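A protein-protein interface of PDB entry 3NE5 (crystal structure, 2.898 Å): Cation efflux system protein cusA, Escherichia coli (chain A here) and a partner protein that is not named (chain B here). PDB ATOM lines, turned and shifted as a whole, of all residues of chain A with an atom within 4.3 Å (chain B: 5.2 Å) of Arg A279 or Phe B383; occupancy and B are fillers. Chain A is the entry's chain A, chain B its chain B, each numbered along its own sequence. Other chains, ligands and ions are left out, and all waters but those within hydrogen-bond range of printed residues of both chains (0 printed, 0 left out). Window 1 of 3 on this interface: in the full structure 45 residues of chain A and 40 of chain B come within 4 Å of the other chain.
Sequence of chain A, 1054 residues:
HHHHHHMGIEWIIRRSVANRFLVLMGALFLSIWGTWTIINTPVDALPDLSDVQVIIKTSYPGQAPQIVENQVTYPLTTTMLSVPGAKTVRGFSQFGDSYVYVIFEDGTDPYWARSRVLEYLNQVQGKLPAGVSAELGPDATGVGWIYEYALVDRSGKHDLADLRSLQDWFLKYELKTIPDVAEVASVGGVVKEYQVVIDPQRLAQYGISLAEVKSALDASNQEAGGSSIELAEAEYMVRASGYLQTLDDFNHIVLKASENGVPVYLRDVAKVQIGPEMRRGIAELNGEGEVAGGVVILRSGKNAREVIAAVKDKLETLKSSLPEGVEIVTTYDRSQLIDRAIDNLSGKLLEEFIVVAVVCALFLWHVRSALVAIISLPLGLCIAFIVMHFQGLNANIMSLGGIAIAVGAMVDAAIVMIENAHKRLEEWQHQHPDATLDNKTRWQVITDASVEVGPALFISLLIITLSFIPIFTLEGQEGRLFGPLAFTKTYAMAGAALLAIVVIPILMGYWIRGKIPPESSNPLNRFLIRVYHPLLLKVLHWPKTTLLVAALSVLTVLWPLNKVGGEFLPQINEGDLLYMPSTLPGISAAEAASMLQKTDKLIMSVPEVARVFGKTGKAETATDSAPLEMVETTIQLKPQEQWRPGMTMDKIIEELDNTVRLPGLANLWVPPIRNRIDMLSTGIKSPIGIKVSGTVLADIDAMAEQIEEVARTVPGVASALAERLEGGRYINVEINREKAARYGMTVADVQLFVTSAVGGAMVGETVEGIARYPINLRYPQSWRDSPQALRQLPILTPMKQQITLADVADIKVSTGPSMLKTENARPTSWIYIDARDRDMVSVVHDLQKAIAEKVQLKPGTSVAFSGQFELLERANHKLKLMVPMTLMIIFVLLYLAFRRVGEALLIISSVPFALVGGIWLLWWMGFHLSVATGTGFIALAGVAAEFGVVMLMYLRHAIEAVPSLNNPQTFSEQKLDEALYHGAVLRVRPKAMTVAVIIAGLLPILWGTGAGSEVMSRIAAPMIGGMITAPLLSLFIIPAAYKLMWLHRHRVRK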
ATOM      1  N   GLY A 189     -29.494 -24.079   8.423  1.00  0.00           N
ATOM      2  CA  GLY A 189     -28.549 -23.519   7.474  1.00  0.00           C
ATOM      3  C   GLY A 189     -28.526 -22.001   7.515  1.00  0.00           C
ATOM      4  O   GLY A 189     -29.345 -21.378   8.193  1.00  0.00           O
ATOM      5  N   VAL A 190     -27.588 -21.408   6.783  1.00  0.00           N
ATOM      6  CA  VAL A 190     -27.431 -19.957   6.757  1.00  0.00           C
ATOM      7  C   VAL A 190     -27.825 -19.356   5.413  1.00  0.00           C
ATOM      8  O   VAL A 190     -27.399 -19.835   4.362  1.00  0.00           O
ATOM      9  CB  VAL A 190     -25.977 -19.546   7.055  1.00  0.00           C
ATOM     10  CG1 VAL A 190     -25.711 -18.128   6.565  1.00  0.00           C
ATOM     11  CG2 VAL A 190     -25.686 -19.668   8.535  1.00  0.00           C
ATOM     12  N   GLU A 277     -27.927 -14.262   7.598  1.00  0.00           N
ATOM     13  CA  GLU A 277     -29.178 -13.575   7.874  1.00  0.00           C
ATOM     14  C   GLU A 277     -29.676 -14.054   9.228  1.00  0.00           C
ATOM     15  O   GLU A 277     -29.146 -15.017   9.779  1.00  0.00           O
ATOM     16  CB  GLU A 277     -30.214 -13.876   6.791  1.00  0.00           C
ATOM     17  CG  GLU A 277     -31.493 -13.061   6.913  1.00  0.00           C
ATOM     18  CD  GLU A 277     -32.611 -13.594   6.039  1.00  0.00           C
ATOM     19  OE1 GLU A 277     -32.719 -14.831   5.897  1.00  0.00           O
ATOM     20  OE2 GLU A 277     -33.386 -12.774   5.500  1.00  0.00           O
ATOM     21  N   MET A 278     -30.683 -13.383   9.773  1.00  0.00           N
ATOM     22  CA  MET A 278     -31.270 -13.841  11.022  1.00  0.00           C
ATOM     23  C   MET A 278     -31.821 -15.245  10.828  1.00  0.00           C
ATOM     24  O   MET A 278     -32.723 -15.461  10.018  1.00  0.00           O
ATOM     25  CB  MET A 278     -32.385 -12.907  11.486  1.00  0.00           C
ATOM     26  CG  MET A 278     -33.040 -13.354  12.781  1.00  0.00           C
ATOM     27  SD  MET A 278     -34.521 -12.413  13.179  1.00  0.00           S
ATOM     28  CE  MET A 278     -34.801 -12.931  14.870  1.00  0.00           C
ATOM     29  N   ARG A 279     -31.265 -16.199  11.565  1.00  0.00           N
ATOM     30  CA  ARG A 279     -31.759 -17.567  11.527  1.00  0.00           C
ATOM     31  C   ARG A 279     -33.157 -17.649  12.129  1.00  0.00           C
ATOM     32  O   ARG A 279     -33.377 -17.229  13.264  1.00  0.00           O
ATOM     33  CB  ARG A 279     -30.810 -18.495  12.288  1.00  0.00           C
ATOM     34  CG  ARG A 279     -29.767 -19.180  11.424  1.00  0.00           C
ATOM     35  CD  ARG A 279     -28.749 -19.912  12.283  1.00  0.00           C
ATOM     36  NE  ARG A 279     -27.575 -19.089  12.551  1.00  0.00           N
ATOM     37  CZ  ARG A 279     -26.363 -19.347  12.071  1.00  0.00           C
ATOM     38  NH1 ARG A 279     -25.346 -18.546  12.356  1.00  0.00           N
ATOM     39  NH2 ARG A 279     -26.166 -20.415  11.314  1.00  0.00           N
ATOM     40  N   ARG A 280     -34.102 -18.178  11.361  1.00  0.00           N
ATOM     41  CA  ARG A 280     -35.441 -18.425  11.885  1.00  0.00           C
ATOM     42  C   ARG A 280     -35.646 -19.913  12.137  1.00  0.00           C
ATOM     43  O   ARG A 280     -36.709 -20.341  12.587  1.00  0.00           O
ATOM     44  CB  ARG A 280     -36.512 -17.863  10.949  1.00  0.00           C
ATOM     45  CG  ARG A 280     -36.043 -17.649   9.525  1.00  0.00           C
ATOM     46  CD  ARG A 280     -36.984 -16.719   8.777  1.00  0.00           C
ATOM     47  NE  ARG A 280     -36.270 -15.924   7.781  1.00  0.00           N
ATOM     48  CZ  ARG A 280     -36.188 -16.234   6.492  1.00  0.00           C
ATOM     49  NH1 ARG A 280     -35.513 -15.450   5.662  1.00  0.00           N
ATOM     50  NH2 ARG A 280     -36.785 -17.323   6.030  1.00  0.00           N
ATOM     51  N   GLY A 281     -34.607 -20.691  11.852  1.00  0.00           N
ATOM     52  CA  GLY A 281     -34.613 -22.120  12.098  1.00  0.00           C
ATOM     53  C   GLY A 281     -33.199 -22.661  12.197  1.00  0.00           C
ATOM     54  O   GLY A 281     -32.325 -22.286  11.413  1.00  0.00           O
ATOM     55  N   ILE A 282     -32.971 -23.541  13.166  1.00  0.00           N
ATOM     56  CA  ILE A 282     -31.655 -24.132  13.371  1.00  0.00           C
ATOM     57  C   ILE A 282     -31.743 -25.655  13.383  1.00  0.00           C
ATOM     58  O   ILE A 282     -32.620 -26.231  14.026  1.00  0.00           O
ATOM     59  CB  ILE A 282     -31.027 -23.642  14.688  1.00  0.00           C
ATOM     60  CG1 ILE A 282     -30.852 -22.122  14.652  1.00  0.00           C
ATOM     61  CG2 ILE A 282     -29.695 -24.329  14.936  1.00  0.00           C
ATOM     62  CD1 ILE A 282     -30.639 -21.493  16.011  1.00  0.00           C
ATOM     63  N   GLU A 290     -23.950 -28.026  13.551  1.00  0.00           N
ATOM     64  CA  GLU A 290     -25.094 -27.417  12.895  1.00  0.00           C
ATOM     65  C   GLU A 290     -25.061 -27.826  11.425  1.00  0.00           C
ATOM     66  O   GLU A 290     -23.987 -27.974  10.841  1.00  0.00           O
ATOM     67  CB  GLU A 290     -25.031 -25.892  13.036  1.00  0.00           C
ATOM     68  CG  GLU A 290     -26.196 -25.136  12.414  1.00  0.00           C
ATOM     69  CD  GLU A 290     -26.008 -23.628  12.462  1.00  0.00           C
ATOM     70  OE1 GLU A 290     -26.241 -22.969  11.428  1.00  0.00           O
ATOM     71  OE2 GLU A 290     -25.621 -23.101  13.528  1.00  0.00           O
ATOM     72  N   LEU A 628     -38.262 -19.813  17.648  1.00  0.00           N
ATOM     73  CA  LEU A 628     -36.867 -20.210  17.803  1.00  0.00           C
ATOM     74  C   LEU A 628     -36.604 -20.743  19.205  1.00  0.00           C
ATOM     75  O   LEU A 628     -35.578 -21.371  19.461  1.00  0.00           O
ATOM     76  CB  LEU A 628     -35.938 -19.035  17.498  1.00  0.00           C
ATOM     77  CG  LEU A 628     -35.512 -18.898  16.038  1.00  0.00           C
ATOM     78  CD1 LEU A 628     -35.216 -17.448  15.699  1.00  0.00           C
ATOM     79  CD2 LEU A 628     -34.298 -19.773  15.773  1.00  0.00           C
ATOM     80  N   GLN B  90     -18.449 -28.866  16.538  1.00  0.00           N
ATOM     81  CA  GLN B  90     -18.562 -28.808  15.088  1.00  0.00           C
ATOM     82  C   GLN B  90     -17.604 -29.808  14.454  1.00  0.00           C
ATOM     83  O   GLN B  90     -16.461 -29.476  14.136  1.00  0.00           O
ATOM     84  CB  GLN B  90     -18.281 -27.395  14.575  1.00  0.00           C
ATOM     85  CG  GLN B  90     -18.364 -27.243  13.061  1.00  0.00           C
ATOM     86  CD  GLN B  90     -19.724 -27.626  12.498  1.00  0.00           C
ATOM     87  OE1 GLN B  90     -20.114 -28.794  12.519  1.00  0.00           O
ATOM     88  NE2 GLN B  90     -20.445 -26.640  11.976  1.00  0.00           N
ATOM     89  N   VAL B  94     -15.406 -28.138   8.815  1.00  0.00           N
ATOM     90  CA  VAL B  94     -15.051 -26.738   9.000  1.00  0.00           C
ATOM     91  C   VAL B  94     -14.396 -26.157   7.747  1.00  0.00           C
ATOM     92  O   VAL B  94     -13.534 -26.792   7.140  1.00  0.00           O
ATOM     93  CB  VAL B  94     -14.107 -26.522  10.186  1.00  0.00           C
ATOM     94  CG1 VAL B  94     -13.875 -25.048  10.396  1.00  0.00           C
ATOM     95  CG2 VAL B  94     -14.674 -27.127  11.451  1.00  0.00           C
ATOM     96  N   PHE B 350     -12.034 -25.032  18.485  1.00  0.00           N
ATOM     97  CA  PHE B 350     -12.226 -23.610  18.217  1.00  0.00           C
ATOM     98  C   PHE B 350     -11.685 -22.766  19.365  1.00  0.00           C
ATOM     99  O   PHE B 350     -12.022 -22.997  20.527  1.00  0.00           O
ATOM    100  CB  PHE B 350     -13.710 -23.298  18.014  1.00  0.00           C
ATOM    101  CG  PHE B 350     -14.236 -23.680  16.658  1.00  0.00           C
ATOM    102  CD1 PHE B 350     -13.517 -24.523  15.828  1.00  0.00           C
ATOM    103  CD2 PHE B 350     -15.469 -23.217  16.230  1.00  0.00           C
ATOM    104  CE1 PHE B 350     -14.009 -24.881  14.584  1.00  0.00           C
ATOM    105  CE2 PHE B 350     -15.968 -23.574  14.990  1.00  0.00           C
ATOM    106  CZ  PHE B 350     -15.237 -24.408  14.165  1.00  0.00           C
ATOM    107  N   VAL B 378     -10.887 -20.255  10.752  1.00  0.00           N
ATOM    108  CA  VAL B 378     -12.112 -20.538  10.018  1.00  0.00           C
ATOM    109  C   VAL B 378     -12.648 -19.276   9.356  1.00  0.00           C
ATOM    110  O   VAL B 378     -12.893 -18.270  10.022  1.00  0.00           O
ATOM    111  CB  VAL B 378     -13.194 -21.168  10.913  1.00  0.00           C
ATOM    112  CG1 VAL B 378     -13.225 -20.491  12.264  1.00  0.00           C
ATOM    113  CG2 VAL B 378     -14.552 -21.067  10.242  1.00  0.00           C
ATOM    114  N   SER B 380     -15.373 -17.818   8.488  1.00  0.00           N
ATOM    115  CA  SER B 380     -16.819 -17.715   8.621  1.00  0.00           C
ATOM    116  C   SER B 380     -17.269 -16.914   9.844  1.00  0.00           C
ATOM    117  O   SER B 380     -16.939 -17.247  10.983  1.00  0.00           O
ATOM    118  CB  SER B 380     -17.450 -19.110   8.630  1.00  0.00           C
ATOM    119  OG  SER B 380     -17.175 -19.799   7.422  1.00  0.00           O
ATOM    120  N   GLY B 381     -18.010 -15.842   9.585  1.00  0.00           N
ATOM    121  CA  GLY B 381     -18.716 -15.120  10.626  1.00  0.00           C
ATOM    122  C   GLY B 381     -20.139 -15.631  10.570  1.00  0.00           C
ATOM    123  O   GLY B 381     -21.042 -15.116  11.230  1.00  0.00           O
ATOM    124  N   LEU B 382     -20.318 -16.664   9.752  1.00  0.00           N
ATOM    125  CA  LEU B 382     -21.607 -17.302   9.542  1.00  0.00           C
ATOM    126  C   LEU B 382     -21.881 -18.300  10.665  1.00  0.00           C
ATOM    127  O   LEU B 382     -22.677 -19.225  10.505  1.00  0.00           O
ATOM    128  CB  LEU B 382     -21.618 -18.022   8.187  1.00  0.00           C
ATOM    129  CG  LEU B 382     -21.180 -17.263   6.925  1.00  0.00           C
ATOM    130  CD1 LEU B 382     -20.691 -18.224   5.849  1.00  0.00           C
ATOM    131  CD2 LEU B 382     -22.291 -16.374   6.379  1.00  0.00           C
ATOM    132  N   PHE B 383     -21.215 -18.108  11.802  1.00  0.00           N
ATOM    133  CA  PHE B 383     -21.313 -19.042  12.924  1.00  0.00           C
ATOM    134  C   PHE B 383     -22.090 -18.471  14.108  1.00  0.00           C
ATOM    135  O   PHE B 383     -22.365 -19.176  15.078  1.00  0.00           O
ATOM    136  CB  PHE B 383     -19.915 -19.482  13.366  1.00  0.00           C
ATOM    137  CG  PHE B 383     -19.300 -20.521  12.474  1.00  0.00           C
ATOM    138  CD1 PHE B 383     -19.653 -20.598  11.138  1.00  0.00           C
ATOM    139  CD2 PHE B 383     -18.357 -21.406  12.965  1.00  0.00           C
ATOM    140  CE1 PHE B 383     -19.090 -21.550  10.309  1.00  0.00           C
ATOM    141  CE2 PHE B 383     -17.787 -22.358  12.142  1.00  0.00           C
ATOM    142  CZ  PHE B 383     -18.154 -22.431  10.811  1.00  0.00           C
ATOM    143  N   LEU B 384     -22.437 -17.191  14.021  1.00  0.00           N
ATOM    144  CA  LEU B 384     -23.254 -16.540  15.038  1.00  0.00           C
ATOM    145  C   LEU B 384     -24.430 -15.862  14.352  1.00  0.00           C
ATOM    146  O   LEU B 384     -24.251 -15.185  13.342  1.00  0.00           O
ATOM    147  CB  LEU B 384     -22.439 -15.505  15.810  1.00  0.00           C
ATOM    148  CG  LEU B 384     -21.091 -15.950  16.371  1.00  0.00           C
ATOM    149  CD1 LEU B 384     -20.036 -15.969  15.280  1.00  0.00           C
ATOM    150  CD2 LEU B 384     -20.669 -15.024  17.492  1.00  0.00           C
ATOM    151  N   ILE B 385     -25.618 -16.005  14.904  1.00  0.00           N
ATOM    152  CA  ILE B 385     -26.770 -15.443  14.242  1.00  0.00           C
ATOM    153  C   ILE B 385     -26.659 -13.929  14.145  1.00  0.00           C
ATOM    154  O   ILE B 385     -26.220 -13.266  15.061  1.00  0.00           O
ATOM    155  CB  ILE B 385     -28.114 -15.962  14.843  1.00  0.00           C
ATOM    156  CG1 ILE B 385     -29.253 -15.759  13.873  1.00  0.00           C
ATOM    157  CG2 ILE B 385     -28.454 -15.319  16.142  1.00  0.00           C
ATOM    158  CD1 ILE B 385     -30.517 -15.537  14.551  1.00  0.00           C
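The guanidinium group (NH1) of Arg A279 sits at hydrogen-bond distance from the backbone carbonyl oxygen (O) of Leu B382 (3.3 Å).
The side-chain carboxylate of Glu A290 lies within salt-bridge range of the guanidinium group of Arg A279 (2.6 Å).
O of Leu B382 touches CG2 of Val A190, 3.6 Å away.
Met A278 touches Ile B385.
Arg A279 touches Phe B383 (NH1 to C, 3.7 Å).
Arg A279 touches Leu B384.
Arg A279 touches Ile B385 (N to CG1, 3.1 Å).
Glu A290 touches Gln B90 (O to NE2, 3.95 Å).
Arg A279 touches four residues of chain B.
Of chain A, only Arg A279 comes within 4 Å of Phe B383.
Printed residues of chain A within 4 Å of Leu B384: Arg A279 (3.5 Å).
Of the printed residues of chain B, Glu A290 touches Gln B90.
Of the printed residues of chain A, Leu B382 touches Val A190 (3.6 Å) and Arg A279 (3.3 Å).
Printed residues of chain B within 4 Å of Val A190: Leu B382.
Of the printed residues of chain B, Met A278 touches Ile B385 (3.8 Å).
Glu A277 touches none of the printed residues of chain B.
Gly B381 touches none of the printed residues of chain A.
Printed residues of chain A that touch a printed residue of chain B: Val A190, Met A278, Arg A279 and Glu A290.
Hydrophobic or aromatic side chains of chain A within 4 Å of the printed part of chain B: Val A190 and Met A278.
Printed residues of chain B that touch a printed residue of chain A: Gln B90, Leu B382, Phe B383, Leu B384 and Ile B385.
Hydrophobic or aromatic side chains of chain B within 4 Å of the printed part of chain A: Leu B382 and Ile B385.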
